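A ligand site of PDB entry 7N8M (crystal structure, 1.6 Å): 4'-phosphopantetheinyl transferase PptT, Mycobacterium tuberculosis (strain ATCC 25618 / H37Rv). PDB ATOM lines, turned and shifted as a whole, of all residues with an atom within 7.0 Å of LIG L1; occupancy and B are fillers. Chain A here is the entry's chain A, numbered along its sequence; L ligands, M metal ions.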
ATOM      1  N   LYS A  78      15.466  12.375 -16.847  1.00  0.00           N
ATOM      2  CA  LYS A  78      14.826  13.460 -17.576  1.00  0.00           C
ATOM      3  C   LYS A  78      13.315  13.490 -17.353  1.00  0.00           C
ATOM      4  O   LYS A  78      12.581  14.020 -18.197  1.00  0.00           O
ATOM      5  CB  LYS A  78      15.140  13.355 -19.069  1.00  0.00           C
ATOM      6  CG  LYS A  78      16.609  13.527 -19.370  1.00  0.00           C
ATOM      7  CD  LYS A  78      17.018  14.949 -19.051  1.00  0.00           C
ATOM      8  CE  LYS A  78      18.437  15.249 -19.500  1.00  0.00           C
ATOM      9  NZ  LYS A  78      18.882  16.544 -18.937  1.00  0.00           N
ATOM     10  N   ILE A 129       7.345  27.333 -30.211  1.00  0.00           N
ATOM     11  CA  ILE A 129       7.054  25.905 -30.341  1.00  0.00           C
ATOM     12  C   ILE A 129       6.870  25.451 -31.777  1.00  0.00           C
ATOM     13  O   ILE A 129       6.634  24.253 -32.004  1.00  0.00           O
ATOM     14  CB  ILE A 129       5.838  25.485 -29.457  1.00  0.00           C
ATOM     15  CG1 ILE A 129       4.506  26.166 -29.859  1.00  0.00           C
ATOM     16  CG2 ILE A 129       6.136  25.741 -27.978  1.00  0.00           C
ATOM     17  CD1 ILE A 129       3.785  25.557 -31.056  1.00  0.00           C
ATOM     18  N   PHE A 153       1.183  22.477 -30.869  1.00  0.00           N
ATOM     19  CA  PHE A 153       1.932  22.296 -29.622  1.00  0.00           C
ATOM     20  C   PHE A 153       1.710  20.895 -29.047  1.00  0.00           C
ATOM     21  O   PHE A 153       2.663  20.201 -28.682  1.00  0.00           O
ATOM     22  CB  PHE A 153       1.527  23.372 -28.605  1.00  0.00           C
ATOM     23  CG  PHE A 153       2.158  23.186 -27.266  1.00  0.00           C
ATOM     24  CD1 PHE A 153       3.550  23.234 -27.126  1.00  0.00           C
ATOM     25  CD2 PHE A 153       1.396  22.895 -26.152  1.00  0.00           C
ATOM     26  CE1 PHE A 153       4.141  23.025 -25.902  1.00  0.00           C
ATOM     27  CE2 PHE A 153       1.997  22.683 -24.915  1.00  0.00           C
ATOM     28  CZ  PHE A 153       3.376  22.743 -24.792  1.00  0.00           C
ATOM     29  N   ALA A 155       0.893  18.181 -30.654  1.00  0.00           N
ATOM     30  CA  ALA A 155       1.579  17.230 -31.506  1.00  0.00           C
ATOM     31  C   ALA A 155       3.074  17.221 -31.215  1.00  0.00           C
ATOM     32  O   ALA A 155       3.703  16.168 -31.216  1.00  0.00           O
ATOM     33  CB  ALA A 155       1.298  17.555 -32.976  1.00  0.00           C
ATOM     34  N   LYS A 156       3.644  18.400 -30.916  1.00  0.00           N
ATOM     35  CA  LYS A 156       5.066  18.459 -30.573  1.00  0.00           C
ATOM     36  C   LYS A 156       5.335  17.710 -29.275  1.00  0.00           C
ATOM     37  O   LYS A 156       6.370  17.048 -29.135  1.00  0.00           O
ATOM     38  CB  LYS A 156       5.546  19.913 -30.415  1.00  0.00           C
ATOM     39  CG  LYS A 156       5.407  20.791 -31.666  1.00  0.00           C
ATOM     40  CD  LYS A 156       6.631  20.727 -32.580  1.00  0.00           C
ATOM     41  CE  LYS A 156       6.347  21.498 -33.866  1.00  0.00           C
ATOM     42  NZ  LYS A 156       7.589  21.772 -34.662  1.00  0.00           N
ATOM     43  N   GLU A 157       4.412  17.801 -28.319  1.00  0.00           N
ATOM     44  CA  GLU A 157       4.603  17.143 -27.022  1.00  0.00           C
ATOM     45  C   GLU A 157       4.461  15.630 -27.155  1.00  0.00           C
ATOM     46  O   GLU A 157       5.267  14.875 -26.596  1.00  0.00           O
ATOM     47  CB  GLU A 157       3.604  17.696 -25.994  1.00  0.00           C
ATOM     48  CG  GLU A 157       3.798  19.193 -25.709  1.00  0.00           C
ATOM     49  CD  GLU A 157       5.188  19.462 -25.199  1.00  0.00           C
ATOM     50  OE1 GLU A 157       5.374  19.364 -23.962  1.00  0.00           O
ATOM     51  OE2 GLU A 157       6.100  19.695 -26.025  1.00  0.00           O
ATOM     52  N   ALA A 158       3.434  15.161 -27.877  1.00  0.00           N
ATOM     53  CA  ALA A 158       3.328  13.712 -28.071  1.00  0.00           C
ATOM     54  C   ALA A 158       4.546  13.188 -28.801  1.00  0.00           C
ATOM     55  O   ALA A 158       5.022  12.086 -28.515  1.00  0.00           O
ATOM     56  CB  ALA A 158       2.043  13.358 -28.836  1.00  0.00           C
ATOM     57  N   THR A 159       5.092  13.979 -29.736  1.00  0.00           N
ATOM     58  CA  THR A 159       6.274  13.554 -30.473  1.00  0.00           C
ATOM     59  C   THR A 159       7.472  13.368 -29.560  1.00  0.00           C
ATOM     60  O   THR A 159       8.170  12.335 -29.612  1.00  0.00           O
ATOM     61  CB  THR A 159       6.605  14.551 -31.585  1.00  0.00           C
ATOM     62  OG1 THR A 159       5.514  14.651 -32.506  1.00  0.00           O
ATOM     63  CG2 THR A 159       7.841  14.039 -32.327  1.00  0.00           C
ATOM     64  N   TYR A 160       7.748  14.367 -28.711  1.00  0.00           N
ATOM     65  CA  TYR A 160       8.858  14.234 -27.776  1.00  0.00           C
ATOM     66  C   TYR A 160       8.691  13.040 -26.849  1.00  0.00           C
ATOM     67  O   TYR A 160       9.655  12.316 -26.568  1.00  0.00           O
ATOM     68  CB  TYR A 160       9.003  15.527 -26.964  1.00  0.00           C
ATOM     69  CG  TYR A 160      10.110  15.505 -25.940  1.00  0.00           C
ATOM     70  CD1 TYR A 160      11.418  15.170 -26.275  1.00  0.00           C
ATOM     71  CD2 TYR A 160       9.833  15.842 -24.610  1.00  0.00           C
ATOM     72  CE1 TYR A 160      12.420  15.163 -25.313  1.00  0.00           C
ATOM     73  CE2 TYR A 160      10.844  15.838 -23.648  1.00  0.00           C
ATOM     74  CZ  TYR A 160      12.130  15.509 -24.009  1.00  0.00           C
ATOM     75  OH  TYR A 160      13.118  15.515 -23.032  1.00  0.00           O
ATOM     76  N   LYS A 161       7.461  12.803 -26.364  1.00  0.00           N
ATOM     77  CA  LYS A 161       7.274  11.717 -25.404  1.00  0.00           C
ATOM     78  C   LYS A 161       7.431  10.355 -26.054  1.00  0.00           C
ATOM     79  O   LYS A 161       7.869   9.413 -25.392  1.00  0.00           O
ATOM     80  CB  LYS A 161       5.901  11.825 -24.730  1.00  0.00           C
ATOM     81  CG  LYS A 161       5.755  13.031 -23.809  1.00  0.00           C
ATOM     82  CD  LYS A 161       4.317  13.055 -23.252  1.00  0.00           C
ATOM     83  CE  LYS A 161       3.959  14.347 -22.562  1.00  0.00           C
ATOM     84  NZ  LYS A 161       2.514  14.262 -22.139  1.00  0.00           N
ATOM     85  N   TRP A 170      17.457  14.921 -26.225  1.00  0.00           N
ATOM     86  CA  TRP A 170      16.583  16.067 -26.419  1.00  0.00           C
ATOM     87  C   TRP A 170      16.003  16.107 -27.828  1.00  0.00           C
ATOM     88  O   TRP A 170      16.673  15.766 -28.803  1.00  0.00           O
ATOM     89  CB  TRP A 170      17.375  17.342 -26.134  1.00  0.00           C
ATOM     90  CG  TRP A 170      16.655  18.618 -26.407  1.00  0.00           C
ATOM     91  CD1 TRP A 170      16.995  19.557 -27.337  1.00  0.00           C
ATOM     92  CD2 TRP A 170      15.496  19.122 -25.737  1.00  0.00           C
ATOM     93  NE1 TRP A 170      16.106  20.609 -27.307  1.00  0.00           N
ATOM     94  CE2 TRP A 170      15.180  20.366 -26.330  1.00  0.00           C
ATOM     95  CE3 TRP A 170      14.687  18.635 -24.700  1.00  0.00           C
ATOM     96  CZ2 TRP A 170      14.083  21.139 -25.918  1.00  0.00           C
ATOM     97  CZ3 TRP A 170      13.608  19.412 -24.288  1.00  0.00           C
ATOM     98  CH2 TRP A 170      13.318  20.643 -24.904  1.00  0.00           C
ATOM     99  N   LEU A 171      14.755  16.558 -27.943  1.00  0.00           N
ATOM    100  CA  LEU A 171      14.156  16.920 -29.223  1.00  0.00           C
ATOM    101  C   LEU A 171      13.543  18.308 -29.051  1.00  0.00           C
ATOM    102  O   LEU A 171      12.606  18.474 -28.263  1.00  0.00           O
ATOM    103  CB  LEU A 171      13.079  15.908 -29.661  1.00  0.00           C
ATOM    104  CG  LEU A 171      12.482  16.128 -31.051  1.00  0.00           C
ATOM    105  CD1 LEU A 171      13.496  15.679 -32.134  1.00  0.00           C
ATOM    106  CD2 LEU A 171      11.157  15.377 -31.198  1.00  0.00           C
ATOM    107  N   GLY A 172      14.116  19.308 -29.724  1.00  0.00           N
ATOM    108  CA  GLY A 172      13.572  20.643 -29.620  1.00  0.00           C
ATOM    109  C   GLY A 172      12.332  20.826 -30.484  1.00  0.00           C
ATOM    110  O   GLY A 172      12.043  20.035 -31.387  1.00  0.00           O
ATOM    111  N   PHE A 173      11.591  21.909 -30.221  1.00  0.00           N
ATOM    112  CA  PHE A 173      10.437  22.227 -31.047  1.00  0.00           C
ATOM    113  C   PHE A 173      10.816  22.486 -32.500  1.00  0.00           C
ATOM    114  O   PHE A 173       9.994  22.285 -33.406  1.00  0.00           O
ATOM    115  CB  PHE A 173       9.701  23.436 -30.464  1.00  0.00           C
ATOM    116  CG  PHE A 173       9.101  23.165 -29.122  1.00  0.00           C
ATOM    117  CD1 PHE A 173       7.894  22.482 -29.031  1.00  0.00           C
ATOM    118  CD2 PHE A 173       9.758  23.522 -27.961  1.00  0.00           C
ATOM    119  CE1 PHE A 173       7.356  22.190 -27.813  1.00  0.00           C
ATOM    120  CE2 PHE A 173       9.210  23.226 -26.721  1.00  0.00           C
ATOM    121  CZ  PHE A 173       8.000  22.557 -26.647  1.00  0.00           C
ATOM    122  N   GLU A 174      12.055  22.926 -32.756  1.00  0.00           N
ATOM    123  CA  GLU A 174      12.516  23.178 -34.110  1.00  0.00           C
ATOM    124  C   GLU A 174      13.088  21.934 -34.789  1.00  0.00           C
ATOM    125  O   GLU A 174      13.498  22.003 -35.956  1.00  0.00           O
ATOM    126  CB  GLU A 174      13.556  24.309 -34.104  1.00  0.00           C
ATOM    127  CG  GLU A 174      14.931  23.938 -33.529  1.00  0.00           C
ATOM    128  CD  GLU A 174      15.003  23.837 -31.996  1.00  0.00           C
ATOM    129  OE1 GLU A 174      13.976  23.969 -31.294  1.00  0.00           O
ATOM    130  OE2 GLU A 174      16.127  23.635 -31.473  1.00  0.00           O
ATOM    131  N   ASP A 175      13.119  20.805 -34.083  1.00  0.00           N
ATOM    132  CA  ASP A 175      13.785  19.608 -34.562  1.00  0.00           C
ATOM    133  C   ASP A 175      12.824  18.624 -35.231  1.00  0.00           C
ATOM    134  O   ASP A 175      13.256  17.553 -35.658  1.00  0.00           O
ATOM    135  CB  ASP A 175      14.505  18.896 -33.409  1.00  0.00           C
ATOM    136  CG  ASP A 175      15.708  19.660 -32.897  1.00  0.00           C
ATOM    137  OD1 ASP A 175      16.293  20.439 -33.662  1.00  0.00           O
ATOM    138  OD2 ASP A 175      16.082  19.456 -31.715  1.00  0.00           O
ATOM    139  N   ALA A 176      11.539  18.933 -35.290  1.00  0.00           N
ATOM    140  CA  ALA A 176      10.577  18.065 -35.946  1.00  0.00           C
ATOM    141  C   ALA A 176       9.571  18.929 -36.689  1.00  0.00           C
ATOM    142  O   ALA A 176       9.041  19.885 -36.127  1.00  0.00           O
ATOM    143  CB  ALA A 176       9.849  17.163 -34.921  1.00  0.00           C
HETATM  144  C1  LIG L   1       8.168  20.174 -21.721  1.00  0.00           C
HETATM  145  C2  LIG L   1       9.027  19.669 -24.004  1.00  0.00           C
HETATM  146  C3  LIG L   1       9.353  19.195 -26.424  1.00  0.00           C
HETATM  147  C4  LIG L   1       9.447  18.777 -28.884  1.00  0.00           C
HETATM  148  C5  LIG L   1       9.322  23.948 -22.062  1.00  0.00           C
HETATM  149  C6  LIG L   1       8.862  22.573 -22.481  1.00  0.00           C
HETATM  150  C7  LIG L   1       8.595  21.496 -21.417  1.00  0.00           C
HETATM  151  C8  LIG L   1       8.792  21.843 -20.091  1.00  0.00           C
HETATM  152  C9  LIG L   1       8.571  20.908 -19.061  1.00  0.00           C
HETATM  153  C10 LIG L   1       8.152  19.601 -19.391  1.00  0.00           C
HETATM  154  C11 LIG L   1       7.935  19.254 -20.730  1.00  0.00           C
HETATM  155  C12 LIG L   1       7.497  17.857 -21.021  1.00  0.00           C
HETATM  156  C13 LIG L   1       8.578  16.854 -21.277  1.00  0.00           C
HETATM  157  N1  LIG L   1       7.986  19.897 -23.103  1.00  0.00           N
HETATM  158  N2  LIG L   1       8.585  19.456 -25.304  1.00  0.00           N
HETATM  159  N3  LIG L   1       8.697  19.027 -27.608  1.00  0.00           N
HETATM  160  N4  LIG L   1      10.666  19.155 -26.317  1.00  0.00           N
HETATM  161  O1  LIG L   1      10.191  19.656 -23.703  1.00  0.00           O
HETATM  162  N1  LG2 L   2       9.966  11.557 -22.019  1.00  0.00           N
HETATM  163  C1  LG2 L   2       8.714  11.001 -21.937  1.00  0.00           C
HETATM  164  N2  LG2 L   2       7.742  11.291 -21.092  1.00  0.00           N
HETATM  165  C2  LG2 L   2       8.066  12.259 -20.183  1.00  0.00           C
HETATM  166  C3  LG2 L   2       9.338  12.916 -20.159  1.00  0.00           C
HETATM  167  C4  LG2 L   2      10.273  12.510 -21.108  1.00  0.00           C
HETATM  168  N3  LG2 L   2      11.546  13.065 -21.175  1.00  0.00           N
HETATM  169  N4  LG2 L   2       9.352  13.861 -19.134  1.00  0.00           N
HETATM  170  C5  LG2 L   2       8.138  13.746 -18.573  1.00  0.00           C
HETATM  171  N5  LG2 L   2       7.328  12.770 -19.181  1.00  0.00           N
HETATM  172  C6  LG2 L   2       5.892  12.396 -18.825  1.00  0.00           C
HETATM  173  C7  LG2 L   2       5.799  12.175 -17.293  1.00  0.00           C
HETATM  174  O1  LG2 L   2       5.192  10.950 -17.089  1.00  0.00           O
HETATM  175  C8  LG2 L   2       4.985  13.463 -16.823  1.00  0.00           C
HETATM  176  O2  LG2 L   2       4.123  13.214 -15.846  1.00  0.00           O
HETATM  177  P1  LG2 L   2       4.659  12.846 -14.230  1.00  0.00           P
HETATM  178  O3  LG2 L   2       5.621  13.965 -14.005  1.00  0.00           O
HETATM  179  O4  LG2 L   2       5.203  11.440 -14.373  1.00  0.00           O
HETATM  180  O5  LG2 L   2       3.343  12.922 -13.451  1.00  0.00           O
HETATM  181  C9  LG2 L   2       4.169  13.668 -18.108  1.00  0.00           C
HETATM  182  O6  LG2 L   2       5.076  13.383 -19.179  1.00  0.00           O
HETATM  183  C10 LG2 L   2       3.623  15.067 -18.124  1.00  0.00           C
HETATM  184  O7  LG2 L   2       2.965  15.205 -19.257  1.00  0.00           O
HETATM  185  P2  LG2 L   2       2.311  16.695 -19.533  1.00  0.00           P
HETATM  186  O8  LG2 L   2       3.560  17.568 -19.621  1.00  0.00           O
HETATM  187  O9  LG2 L   2       1.398  16.910 -18.353  1.00  0.00           O
HETATM  188  O10 LG2 L   2       1.615  16.586 -20.883  1.00  0.00           O
HETATM  189 MG    MG M   1       1.491  18.200 -22.095  1.00  0.00          MG
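Residues that only touch LIG L1: Tyr 160 (3.4 Å), Trp 170 (3.4 Å), Gly 172 (3.8 Å) and Phe 173 (3.4 Å).
Within 4 Å of LIG L1: Lys 156, Glu 157, Tyr 160, Trp 170, Leu 171, Gly 172 and Phe 173.
The nearest printed residue that does not touch LIG L1 is Lys 161 (5.2 Å).
A nitrogen (N3) of LG2 L2 lies within hydrogen-bond range of the backbone carbonyl oxygen (O) of Lys 78, 3.3 Å away.
A nitrogen (N3) of LG2 L2 is in hydrogen-bond range of the side-chain hydroxyl (OH) of Tyr 160 (3.5 Å).
A nitrogen (N1) of LIG L1 sits at hydrogen-bond distance from the side-chain carboxylate (OE1) of Glu 157 (2.8 Å).
The backbone carbonyl oxygen (O) of Lys 156 is in hydrogen-bond range of a nitrogen (N3) of LIG L1 (3.4 Å).
N4 of LIG L1 lies within hydrogen-bond range of O of Leu 171, 2.8 Å away.
O7 of LG2 L2 sits at hydrogen-bond distance from NZ of Lys 161 (3.1 Å).
The backbone carbonyl oxygen of Ala 176 sits at hydrogen-bond distance from the side-chain amino group of Lys 156 (2.8 Å).
NZ of Lys 156 is in hydrogen-bond range of O of Phe 173, at 2.8 Å.
N of Gly 172 sits at hydrogen-bond distance from OD2 of Asp 175.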
